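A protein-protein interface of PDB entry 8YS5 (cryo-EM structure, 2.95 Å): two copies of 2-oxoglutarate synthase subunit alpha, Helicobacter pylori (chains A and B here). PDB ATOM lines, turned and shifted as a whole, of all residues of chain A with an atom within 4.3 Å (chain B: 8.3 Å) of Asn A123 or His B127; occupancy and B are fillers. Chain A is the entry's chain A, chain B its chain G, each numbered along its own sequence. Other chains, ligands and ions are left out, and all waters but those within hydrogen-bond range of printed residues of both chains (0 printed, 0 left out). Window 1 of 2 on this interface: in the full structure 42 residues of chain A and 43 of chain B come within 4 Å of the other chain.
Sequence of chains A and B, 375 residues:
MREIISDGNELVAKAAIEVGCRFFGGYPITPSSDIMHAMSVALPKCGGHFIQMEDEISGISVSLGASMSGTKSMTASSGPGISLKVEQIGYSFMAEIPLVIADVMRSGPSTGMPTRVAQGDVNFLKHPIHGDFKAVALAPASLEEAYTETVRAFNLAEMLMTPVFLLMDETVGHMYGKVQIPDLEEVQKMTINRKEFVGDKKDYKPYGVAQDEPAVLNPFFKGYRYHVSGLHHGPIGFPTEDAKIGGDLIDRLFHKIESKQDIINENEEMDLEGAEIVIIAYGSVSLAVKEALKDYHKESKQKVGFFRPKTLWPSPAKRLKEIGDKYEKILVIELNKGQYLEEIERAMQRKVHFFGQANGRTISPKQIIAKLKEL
Of the 10 printed residues of chain A, 7 touch a printed residue of chain B.
Printed residues of chain A that touch a printed residue of chain B: Asp A121, Asn A123, Phe A124, Lys A126, His A127, Gln A339 and Glu A342.
Hydrophobic or aromatic side chains of chain A that line the printed part of chain B: Phe A124 and His A127.
Of the 20 printed residues of chain B, 8 touch a printed residue of chain A.
Printed residues of chain B that touch a printed residue of chain A: Asn B123, Lys B126, His B127, Pro B128, Ile B129, His B130, Gly B131 and Glu B342.
Among the printed residues, 11 pairs touch across the chains.
Asn A123 touches His B127, and with the chains exchanged His A127 touches Asn B123.
Lys A126 touches Glu B342, and with the chains exchanged Glu A342 touches Lys B126.
Positions printed for both chains: 121, 122, 123, 124, 125, 126, 127, 313 and 342.
NZ of Lys B126 lies within salt-bridge range of OE1 of Glu A342, at 3.5 Å.
The side-chain carboxylate (OE1) of Glu B342 is in salt-bridge range of the side-chain amino group (NZ) of Lys A126 (3.6 Å).
OD1 of Asp A121 sits at hydrogen-bond distance from N of Gly B131, 3.3 Å away.
The backbone carbonyl oxygen (O) of Gln A339 sits close to the side-chain amide oxygen (OD1) of Asn A123.
The backbone carbonyl oxygen of Ile B129 sits at hydrogen-bond distance from a ring nitrogen (ND1) of His B127 (3.0 Å).
A ring nitrogen (NE2) of His B127 lies close to the backbone carbonyl oxygen of Gly B131 (3.1 Å).
Of chain B, only His B127 comes within 4 Å of Asn A123.
His B127 touches two residues of chain A.
Of the printed residues of chain B, Asp A121 touches His B130 (3.6 Å) and Gly B131 (3.3 Å).
Of the printed residues of chain A, Lys B126 touches Glu A342 (3.5 Å).
Of the printed residues of chain A, Pro B128 touches Phe A124.
The nearest residue of chain B that does not touch Asn A123 is Lys B126 (5.0 Å).
The nearest printed residue of chain A that does not touch Ile B129 is Asn A123 (6.2 Å).
His B130 touches Asp A121.
His B127 touches Asn A123 (CD2 to CB, 3.9 Å).
Phe A124 touches Pro B128 (CE1 to O, 3.1 Å).
Phe A124 touches Ile B129.
Phe A124 touches His B130 (CD2 to CB, 3.97 Å).
Asn B123 touches His A127 (CB to CD2, 3.96 Å).
His B127 touches Gln A339 (NE2 to OE1, 3.6 Å).
Gly B131 touches Gln A339.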
ATOM      1  N   ASP A 121      -2.539   9.275 -31.483  1.00  0.00           N
ATOM      2  CA  ASP A 121      -3.112   8.193 -30.689  1.00  0.00           C
ATOM      3  C   ASP A 121      -2.292   6.910 -30.808  1.00  0.00           C
ATOM      4  O   ASP A 121      -2.841   5.810 -30.878  1.00  0.00           O
ATOM      5  CB  ASP A 121      -4.560   7.933 -31.094  1.00  0.00           C
ATOM      6  CG  ASP A 121      -5.416   9.183 -31.042  1.00  0.00           C
ATOM      7  OD1 ASP A 121      -4.962  10.196 -30.471  1.00  0.00           O
ATOM      8  OD2 ASP A 121      -6.547   9.152 -31.572  1.00  0.00           O
ATOM      9  N   VAL A 122      -0.967   7.036 -30.835  1.00  0.00           N
ATOM     10  CA  VAL A 122      -0.091   5.877 -30.966  1.00  0.00           C
ATOM     11  C   VAL A 122       0.421   5.466 -29.592  1.00  0.00           C
ATOM     12  O   VAL A 122       0.190   4.337 -29.141  1.00  0.00           O
ATOM     13  CB  VAL A 122       1.075   6.168 -31.925  1.00  0.00           C
ATOM     14  CG1 VAL A 122       1.989   4.961 -32.024  1.00  0.00           C
ATOM     15  CG2 VAL A 122       0.543   6.552 -33.293  1.00  0.00           C
ATOM     16  N   ASN A 123       1.126   6.377 -28.916  1.00  0.00           N
ATOM     17  CA  ASN A 123       1.597   6.086 -27.568  1.00  0.00           C
ATOM     18  C   ASN A 123       0.438   5.918 -26.598  1.00  0.00           C
ATOM     19  O   ASN A 123       0.575   5.229 -25.581  1.00  0.00           O
ATOM     20  CB  ASN A 123       2.538   7.188 -27.085  1.00  0.00           C
ATOM     21  CG  ASN A 123       3.996   6.782 -27.155  1.00  0.00           C
ATOM     22  OD1 ASN A 123       4.342   5.765 -27.758  1.00  0.00           O
ATOM     23  ND2 ASN A 123       4.861   7.574 -26.536  1.00  0.00           N
ATOM     24  N   PHE A 124      -0.702   6.548 -26.885  1.00  0.00           N
ATOM     25  CA  PHE A 124      -1.878   6.366 -26.043  1.00  0.00           C
ATOM     26  C   PHE A 124      -2.359   4.922 -26.078  1.00  0.00           C
ATOM     27  O   PHE A 124      -2.636   4.328 -25.030  1.00  0.00           O
ATOM     28  CB  PHE A 124      -2.990   7.315 -26.493  1.00  0.00           C
ATOM     29  CG  PHE A 124      -4.323   7.043 -25.852  1.00  0.00           C
ATOM     30  CD1 PHE A 124      -4.428   6.843 -24.484  1.00  0.00           C
ATOM     31  CD2 PHE A 124      -5.471   6.986 -26.621  1.00  0.00           C
ATOM     32  CE1 PHE A 124      -5.654   6.592 -23.902  1.00  0.00           C
ATOM     33  CE2 PHE A 124      -6.697   6.736 -26.042  1.00  0.00           C
ATOM     34  CZ  PHE A 124      -6.789   6.539 -24.681  1.00  0.00           C
ATOM     35  N   LEU A 125      -2.454   4.337 -27.272  1.00  0.00           N
ATOM     36  CA  LEU A 125      -2.925   2.965 -27.402  1.00  0.00           C
ATOM     37  C   LEU A 125      -1.815   1.937 -27.242  1.00  0.00           C
ATOM     38  O   LEU A 125      -2.105   0.736 -27.234  1.00  0.00           O
ATOM     39  CB  LEU A 125      -3.629   2.773 -28.745  1.00  0.00           C
ATOM     40  CG  LEU A 125      -4.957   3.524 -28.861  1.00  0.00           C
ATOM     41  CD1 LEU A 125      -5.741   3.036 -30.057  1.00  0.00           C
ATOM     42  CD2 LEU A 125      -5.777   3.375 -27.590  1.00  0.00           C
ATOM     43  N   LYS A 126      -0.560   2.371 -27.123  1.00  0.00           N
ATOM     44  CA  LYS A 126       0.505   1.440 -26.768  1.00  0.00           C
ATOM     45  C   LYS A 126       0.265   0.838 -25.390  1.00  0.00           C
ATOM     46  O   LYS A 126       0.526  -0.349 -25.165  1.00  0.00           O
ATOM     47  CB  LYS A 126       1.859   2.144 -26.814  1.00  0.00           C
ATOM     48  CG  LYS A 126       3.027   1.268 -26.398  1.00  0.00           C
ATOM     49  CD  LYS A 126       4.217   2.105 -25.966  1.00  0.00           C
ATOM     50  CE  LYS A 126       5.462   1.252 -25.816  1.00  0.00           C
ATOM     51  NZ  LYS A 126       5.171   0.000 -25.069  1.00  0.00           N
ATOM     52  N   HIS A 127      -0.241   1.645 -24.456  1.00  0.00           N
ATOM     53  CA  HIS A 127      -0.490   1.201 -23.083  1.00  0.00           C
ATOM     54  C   HIS A 127      -1.617   2.042 -22.499  1.00  0.00           C
ATOM     55  O   HIS A 127      -1.396   2.910 -21.648  1.00  0.00           O
ATOM     56  CB  HIS A 127       0.781   1.315 -22.246  1.00  0.00           C
ATOM     57  CG  HIS A 127       0.724   0.579 -20.946  1.00  0.00           C
ATOM     58  ND1 HIS A 127      -0.283   0.768 -20.025  1.00  0.00           N
ATOM     59  CD2 HIS A 127       1.555  -0.346 -20.411  1.00  0.00           C
ATOM     60  CE1 HIS A 127      -0.071  -0.007 -18.979  1.00  0.00           C
ATOM     61  NE2 HIS A 127       1.037  -0.695 -19.187  1.00  0.00           N
ATOM     62  N   TRP A 313       2.053  -2.325 -32.975  1.00  0.00           N
ATOM     63  CA  TRP A 313       2.346  -3.039 -31.748  1.00  0.00           C
ATOM     64  C   TRP A 313       1.952  -4.505 -31.872  1.00  0.00           C
ATOM     65  O   TRP A 313       0.859  -4.813 -32.356  1.00  0.00           O
ATOM     66  CB  TRP A 313       1.610  -2.412 -30.554  1.00  0.00           C
ATOM     67  CG  TRP A 313       1.767  -0.930 -30.477  1.00  0.00           C
ATOM     68  CD1 TRP A 313       0.808   0.008 -30.721  1.00  0.00           C
ATOM     69  CD2 TRP A 313       2.956  -0.209 -30.136  1.00  0.00           C
ATOM     70  NE1 TRP A 313       1.325   1.269 -30.552  1.00  0.00           N
ATOM     71  CE2 TRP A 313       2.643   1.163 -30.192  1.00  0.00           C
ATOM     72  CE3 TRP A 313       4.254  -0.591 -29.787  1.00  0.00           C
ATOM     73  CZ2 TRP A 313       3.581   2.154 -29.913  1.00  0.00           C
ATOM     74  CZ3 TRP A 313       5.183   0.394 -29.511  1.00  0.00           C
ATOM     75  CH2 TRP A 313       4.842   1.749 -29.576  1.00  0.00           C
ATOM     76  N   GLN A 339       6.197  10.465 -30.572  1.00  0.00           N
ATOM     77  CA  GLN A 339       5.899   9.492 -29.528  1.00  0.00           C
ATOM     78  C   GLN A 339       6.176   8.057 -29.952  1.00  0.00           C
ATOM     79  O   GLN A 339       6.439   7.211 -29.090  1.00  0.00           O
ATOM     80  CB  GLN A 339       4.441   9.620 -29.074  1.00  0.00           C
ATOM     81  CG  GLN A 339       3.414   9.204 -30.103  1.00  0.00           C
ATOM     82  CD  GLN A 339       2.138  10.011 -29.996  1.00  0.00           C
ATOM     83  OE1 GLN A 339       2.039  10.936 -29.192  1.00  0.00           O
ATOM     84  N   GLU A 342      10.206   7.202 -29.838  1.00  0.00           N
ATOM     85  CA  GLU A 342      10.816   6.663 -28.628  1.00  0.00           C
ATOM     86  C   GLU A 342      11.079   5.169 -28.754  1.00  0.00           C
ATOM     87  O   GLU A 342      12.130   4.681 -28.332  1.00  0.00           O
ATOM     88  CB  GLU A 342       9.926   6.951 -27.421  1.00  0.00           C
ATOM     89  CG  GLU A 342       9.701   8.427 -27.161  1.00  0.00           C
ATOM     90  CD  GLU A 342       8.736   8.674 -26.023  1.00  0.00           C
ATOM     91  OE1 GLU A 342       8.302   7.690 -25.389  1.00  0.00           O
ATOM     92  N   VAL B  86      -9.179  10.114 -17.365  1.00  0.00           N
ATOM     93  CA  VAL B  86      -8.263  10.506 -18.431  1.00  0.00           C
ATOM     94  C   VAL B  86      -8.938  11.371 -19.486  1.00  0.00           C
ATOM     95  O   VAL B  86      -8.256  12.074 -20.237  1.00  0.00           O
ATOM     96  CB  VAL B  86      -7.630   9.253 -19.074  1.00  0.00           C
ATOM     97  CG1 VAL B  86      -7.025   8.362 -18.006  1.00  0.00           C
ATOM     98  CG2 VAL B  86      -8.660   8.491 -19.888  1.00  0.00           C
ATOM     99  N   ASP B 121       1.043   1.526 -12.882  1.00  0.00           N
ATOM    100  CA  ASP B 121       0.528   2.800 -13.368  1.00  0.00           C
ATOM    101  C   ASP B 121       1.639   3.799 -13.680  1.00  0.00           C
ATOM    102  O   ASP B 121       1.473   5.002 -13.447  1.00  0.00           O
ATOM    103  CB  ASP B 121      -0.451   3.400 -12.359  1.00  0.00           C
ATOM    104  CG  ASP B 121      -1.513   2.416 -11.919  1.00  0.00           C
ATOM    105  OD1 ASP B 121      -1.477   1.254 -12.375  1.00  0.00           O
ATOM    106  OD2 ASP B 121      -2.389   2.804 -11.119  1.00  0.00           O
ATOM    107  N   VAL B 122       2.770   3.327 -14.197  1.00  0.00           N
ATOM    108  CA  VAL B 122       3.875   4.210 -14.552  1.00  0.00           C
ATOM    109  C   VAL B 122       3.808   4.526 -16.040  1.00  0.00           C
ATOM    110  O   VAL B 122       3.684   5.691 -16.436  1.00  0.00           O
ATOM    111  CB  VAL B 122       5.227   3.582 -14.177  1.00  0.00           C
ATOM    112  CG1 VAL B 122       6.348   4.589 -14.369  1.00  0.00           C
ATOM    113  CG2 VAL B 122       5.188   3.093 -12.745  1.00  0.00           C
ATOM    114  N   ASN B 123       3.889   3.487 -16.876  1.00  0.00           N
ATOM    115  CA  ASN B 123       3.745   3.692 -18.314  1.00  0.00           C
ATOM    116  C   ASN B 123       2.346   4.173 -18.667  1.00  0.00           C
ATOM    117  O   ASN B 123       2.157   4.829 -19.698  1.00  0.00           O
ATOM    118  CB  ASN B 123       4.072   2.402 -19.065  1.00  0.00           C
ATOM    119  CG  ASN B 123       5.516   2.340 -19.516  1.00  0.00           C
ATOM    120  OD1 ASN B 123       6.329   3.189 -19.155  1.00  0.00           O
ATOM    121  ND2 ASN B 123       5.843   1.332 -20.317  1.00  0.00           N
ATOM    122  N   PHE B 124       1.355   3.850 -17.833  1.00  0.00           N
ATOM    123  CA  PHE B 124       0.003   4.351 -18.057  1.00  0.00           C
ATOM    124  C   PHE B 124      -0.054   5.862 -17.876  1.00  0.00           C
ATOM    125  O   PHE B 124      -0.602   6.578 -18.722  1.00  0.00           O
ATOM    126  CB  PHE B 124      -0.975   3.652 -17.110  1.00  0.00           C
ATOM    127  CG  PHE B 124      -2.337   4.288 -17.059  1.00  0.00           C
ATOM    128  CD1 PHE B 124      -3.005   4.636 -18.220  1.00  0.00           C
ATOM    129  CD2 PHE B 124      -2.951   4.532 -15.841  1.00  0.00           C
ATOM    130  CE1 PHE B 124      -4.256   5.220 -18.168  1.00  0.00           C
ATOM    131  CE2 PHE B 124      -4.199   5.114 -15.785  1.00  0.00           C
ATOM    132  CZ  PHE B 124      -4.853   5.459 -16.949  1.00  0.00           C
ATOM    133  N   LEU B 125       0.514   6.365 -16.781  1.00  0.00           N
ATOM    134  CA  LEU B 125       0.497   7.799 -16.517  1.00  0.00           C
ATOM    135  C   LEU B 125       1.572   8.555 -17.283  1.00  0.00           C
ATOM    136  O   LEU B 125       1.592   9.788 -17.229  1.00  0.00           O
ATOM    137  CB  LEU B 125       0.644   8.063 -15.019  1.00  0.00           C
ATOM    138  CG  LEU B 125      -0.545   7.634 -14.159  1.00  0.00           C
ATOM    139  CD1 LEU B 125      -0.577   8.426 -12.872  1.00  0.00           C
ATOM    140  CD2 LEU B 125      -1.853   7.802 -14.915  1.00  0.00           C
ATOM    141  N   LYS B 126       2.467   7.853 -17.981  1.00  0.00           N
ATOM    142  CA  LYS B 126       3.390   8.536 -18.879  1.00  0.00           C
ATOM    143  C   LYS B 126       2.640   9.237 -20.005  1.00  0.00           C
ATOM    144  O   LYS B 126       3.034  10.325 -20.442  1.00  0.00           O
ATOM    145  CB  LYS B 126       4.402   7.543 -19.449  1.00  0.00           C
ATOM    146  CG  LYS B 126       5.393   8.154 -20.422  1.00  0.00           C
ATOM    147  CD  LYS B 126       5.781   7.169 -21.510  1.00  0.00           C
ATOM    148  CE  LYS B 126       7.156   7.481 -22.071  1.00  0.00           C
ATOM    149  NZ  LYS B 126       7.374   8.947 -22.212  1.00  0.00           N
ATOM    150  N   HIS B 127       1.553   8.633 -20.480  1.00  0.00           N
ATOM    151  CA  HIS B 127       0.780   9.170 -21.592  1.00  0.00           C
ATOM    152  C   HIS B 127      -0.655   8.657 -21.518  1.00  0.00           C
ATOM    153  O   HIS B 127      -1.032   7.762 -22.284  1.00  0.00           O
ATOM    154  CB  HIS B 127       1.428   8.781 -22.920  1.00  0.00           C
ATOM    155  CG  HIS B 127       1.007   9.632 -24.076  1.00  0.00           C
ATOM    156  ND1 HIS B 127      -0.313   9.796 -24.437  1.00  0.00           N
ATOM    157  CD2 HIS B 127       1.732  10.360 -24.957  1.00  0.00           C
ATOM    158  CE1 HIS B 127      -0.382  10.591 -25.490  1.00  0.00           C
ATOM    159  NE2 HIS B 127       0.844  10.948 -25.825  1.00  0.00           N
ATOM    160  N   PRO B 128      -1.480   9.188 -20.611  1.00  0.00           N
ATOM    161  CA  PRO B 128      -2.828   8.637 -20.425  1.00  0.00           C
ATOM    162  C   PRO B 128      -3.871   9.198 -21.381  1.00  0.00           C
ATOM    163  O   PRO B 128      -4.875   8.536 -21.658  1.00  0.00           O
ATOM    164  CB  PRO B 128      -3.153   9.011 -18.976  1.00  0.00           C
ATOM    165  CG  PRO B 128      -2.404  10.277 -18.753  1.00  0.00           C
ATOM    166  CD  PRO B 128      -1.164  10.224 -19.610  1.00  0.00           C
ATOM    167  N   ILE B 129      -3.658  10.409 -21.885  1.00  0.00           N
ATOM    168  CA  ILE B 129      -4.642  11.083 -22.716  1.00  0.00           C
ATOM    169  C   ILE B 129      -4.301  10.863 -24.183  1.00  0.00           C
ATOM    170  O   ILE B 129      -3.192  10.460 -24.541  1.00  0.00           O
ATOM    171  CB  ILE B 129      -4.729  12.590 -22.394  1.00  0.00           C
ATOM    172  CG1 ILE B 129      -3.569  13.339 -23.049  1.00  0.00           C
ATOM    173  CG2 ILE B 129      -4.728  12.812 -20.893  1.00  0.00           C
ATOM    174  CD1 ILE B 129      -3.861  14.794 -23.336  1.00  0.00           C
ATOM    175  N   HIS B 130      -5.278  11.122 -25.049  1.00  0.00           N
ATOM    176  CA  HIS B 130      -5.044  11.066 -26.482  1.00  0.00           C
ATOM    177  C   HIS B 130      -4.393  12.360 -26.963  1.00  0.00           C
ATOM    178  O   HIS B 130      -4.386  13.380 -26.268  1.00  0.00           O
ATOM    179  CB  HIS B 130      -6.349  10.811 -27.236  1.00  0.00           C
ATOM    180  CG  HIS B 130      -7.305  11.964 -27.203  1.00  0.00           C
ATOM    181  ND1 HIS B 130      -7.459  12.834 -28.261  1.00  0.00           N
ATOM    182  CD2 HIS B 130      -8.165  12.382 -26.244  1.00  0.00           C
ATOM    183  CE1 HIS B 130      -8.366  13.742 -27.952  1.00  0.00           C
ATOM    184  NE2 HIS B 130      -8.811  13.489 -26.734  1.00  0.00           N
ATOM    185  N   GLY B 131      -3.843  12.310 -28.170  1.00  0.00           N
ATOM    186  CA  GLY B 131      -3.082  13.432 -28.676  1.00  0.00           C
ATOM    187  C   GLY B 131      -1.712  13.513 -28.024  1.00  0.00           C
ATOM    188  O   GLY B 131      -1.130  12.511 -27.600  1.00  0.00           O
ATOM    189  N   ASP B 132      -1.192  14.732 -27.952  1.00  0.00           N
ATOM    190  CA  ASP B 132       0.096  14.979 -27.321  1.00  0.00           C
ATOM    191  C   ASP B 132      -0.091  15.306 -25.845  1.00  0.00           C
ATOM    192  O   ASP B 132      -1.136  15.810 -25.428  1.00  0.00           O
ATOM    193  CB  ASP B 132       0.830  16.118 -28.026  1.00  0.00           C
ATOM    194  CG  ASP B 132       0.951  15.893 -29.519  1.00  0.00           C
ATOM    195  OD1 ASP B 132       1.795  15.069 -29.930  1.00  0.00           O
ATOM    196  OD2 ASP B 132       0.199  16.536 -30.281  1.00  0.00           O
ATOM    197  N   PHE B 133       0.940  15.017 -25.054  1.00  0.00           N
ATOM    198  CA  PHE B 133       0.855  15.196 -23.612  1.00  0.00           C
ATOM    199  C   PHE B 133       2.254  15.186 -23.015  1.00  0.00           C
ATOM    200  O   PHE B 133       3.105  14.395 -23.427  1.00  0.00           O
ATOM    201  CB  PHE B 133      -0.001  14.099 -22.971  1.00  0.00           C
ATOM    202  CG  PHE B 133      -0.298  14.330 -21.517  1.00  0.00           C
ATOM    203  CD1 PHE B 133      -1.034  15.429 -21.114  1.00  0.00           C
ATOM    204  CD2 PHE B 133       0.150  13.442 -20.557  1.00  0.00           C
ATOM    205  CE1 PHE B 133      -1.312  15.641 -19.777  1.00  0.00           C
ATOM    206  CE2 PHE B 133      -0.126  13.650 -19.221  1.00  0.00           C
ATOM    207  CZ  PHE B 133      -0.857  14.751 -18.830  1.00  0.00           C
ATOM    208  N   LYS B 134       2.480  16.069 -22.044  1.00  0.00           N
ATOM    209  CA  LYS B 134       3.719  16.115 -21.272  1.00  0.00           C
ATOM    210  C   LYS B 134       3.358  15.905 -19.809  1.00  0.00           C
ATOM    211  O   LYS B 134       2.774  16.790 -19.174  1.00  0.00           O
ATOM    212  CB  LYS B 134       4.449  17.442 -21.475  1.00  0.00           C
ATOM    213  CG  LYS B 134       5.842  17.472 -20.877  1.00  0.00           C
ATOM    214  CD  LYS B 134       6.832  16.732 -21.757  1.00  0.00           C
ATOM    215  CE  LYS B 134       8.259  16.940 -21.286  1.00  0.00           C
ATOM    216  NZ  LYS B 134       9.235  16.270 -22.186  1.00  0.00           N
ATOM    217  N   ALA B 135       3.709  14.741 -19.274  1.00  0.00           N
ATOM    218  CA  ALA B 135       3.276  14.343 -17.944  1.00  0.00           C
ATOM    219  C   ALA B 135       4.281  14.771 -16.885  1.00  0.00           C
ATOM    220  O   ALA B 135       5.496  14.715 -17.102  1.00  0.00           O
ATOM    221  CB  ALA B 135       3.070  12.829 -17.879  1.00  0.00           C
ATOM    222  N   PHE B 165       0.500  14.614 -11.093  1.00  0.00           N
ATOM    223  CA  PHE B 165       0.156  13.350 -10.463  1.00  0.00           C
ATOM    224  C   PHE B 165       1.030  13.098  -9.242  1.00  0.00           C
ATOM    225  O   PHE B 165       2.196  13.495  -9.190  1.00  0.00           O
ATOM    226  CB  PHE B 165       0.307  12.192 -11.449  1.00  0.00           C
ATOM    227  CG  PHE B 165      -0.470  12.369 -12.722  1.00  0.00           C
ATOM    228  CD1 PHE B 165      -1.810  12.034 -12.781  1.00  0.00           C
ATOM    229  CD2 PHE B 165       0.141  12.862 -13.860  1.00  0.00           C
ATOM    230  CE1 PHE B 165      -2.527  12.193 -13.949  1.00  0.00           C
ATOM    231  CE2 PHE B 165      -0.570  13.023 -15.032  1.00  0.00           C
ATOM    232  CZ  PHE B 165      -1.905  12.688 -15.076  1.00  0.00           C
ATOM    233  N   PHE B 254       4.523  22.181 -24.450  1.00  0.00           N
ATOM    234  CA  PHE B 254       5.664  21.312 -24.165  1.00  0.00           C
ATOM    235  C   PHE B 254       6.834  22.097 -23.579  1.00  0.00           C
ATOM    236  O   PHE B 254       7.480  21.641 -22.625  1.00  0.00           O
ATOM    237  CB  PHE B 254       6.092  20.574 -25.431  1.00  0.00           C
ATOM    238  CG  PHE B 254       5.428  19.242 -25.610  1.00  0.00           C
ATOM    239  CD1 PHE B 254       4.054  19.151 -25.745  1.00  0.00           C
ATOM    240  CD2 PHE B 254       6.176  18.080 -25.642  1.00  0.00           C
ATOM    241  CE1 PHE B 254       3.442  17.926 -25.909  1.00  0.00           C
ATOM    242  CE2 PHE B 254       5.568  16.852 -25.805  1.00  0.00           C
ATOM    243  CZ  PHE B 254       4.200  16.776 -25.939  1.00  0.00           C
ATOM    244  N   TRP B 313       8.426  11.302 -14.161  1.00  0.00           N
ATOM    245  CA  TRP B 313       8.288  12.004 -15.423  1.00  0.00           C
ATOM    246  C   TRP B 313       8.305  13.513 -15.206  1.00  0.00           C
ATOM    247  O   TRP B 313       7.661  14.009 -14.274  1.00  0.00           O
ATOM    248  CB  TRP B 313       6.991  11.608 -16.137  1.00  0.00           C
ATOM    249  CG  TRP B 313       6.764  10.130 -16.182  1.00  0.00           C
ATOM    250  CD1 TRP B 313       5.850   9.420 -15.461  1.00  0.00           C
ATOM    251  CD2 TRP B 313       7.464   9.179 -16.990  1.00  0.00           C
ATOM    252  NE1 TRP B 313       5.936   8.086 -15.770  1.00  0.00           N
ATOM    253  CE2 TRP B 313       6.920   7.911 -16.707  1.00  0.00           C
ATOM    254  CE3 TRP B 313       8.498   9.275 -17.926  1.00  0.00           C
ATOM    255  CZ2 TRP B 313       7.377   6.750 -17.326  1.00  0.00           C
ATOM    256  CZ3 TRP B 313       8.948   8.122 -18.538  1.00  0.00           C
ATOM    257  CH2 TRP B 313       8.388   6.876 -18.236  1.00  0.00           C
ATOM    258  N   GLU B 342      11.792   0.461 -19.879  1.00  0.00           N
ATOM    259  CA  GLU B 342      11.887   0.940 -21.253  1.00  0.00           C
ATOM    260  C   GLU B 342      12.576   2.296 -21.324  1.00  0.00           C
ATOM    261  O   GLU B 342      13.425   2.518 -22.191  1.00  0.00           O
ATOM    262  CB  GLU B 342      10.494   1.007 -21.877  1.00  0.00           C
ATOM    263  CG  GLU B 342       9.625  -0.201 -21.568  1.00  0.00           C
ATOM    264  CD  GLU B 342       8.550  -0.430 -22.608  1.00  0.00           C
ATOM    265  OE1 GLU B 342       8.469   0.367 -23.566  1.00  0.00           O
ATOM    266  OE2 GLU B 342       7.786  -1.408 -22.469  1.00  0.00           O
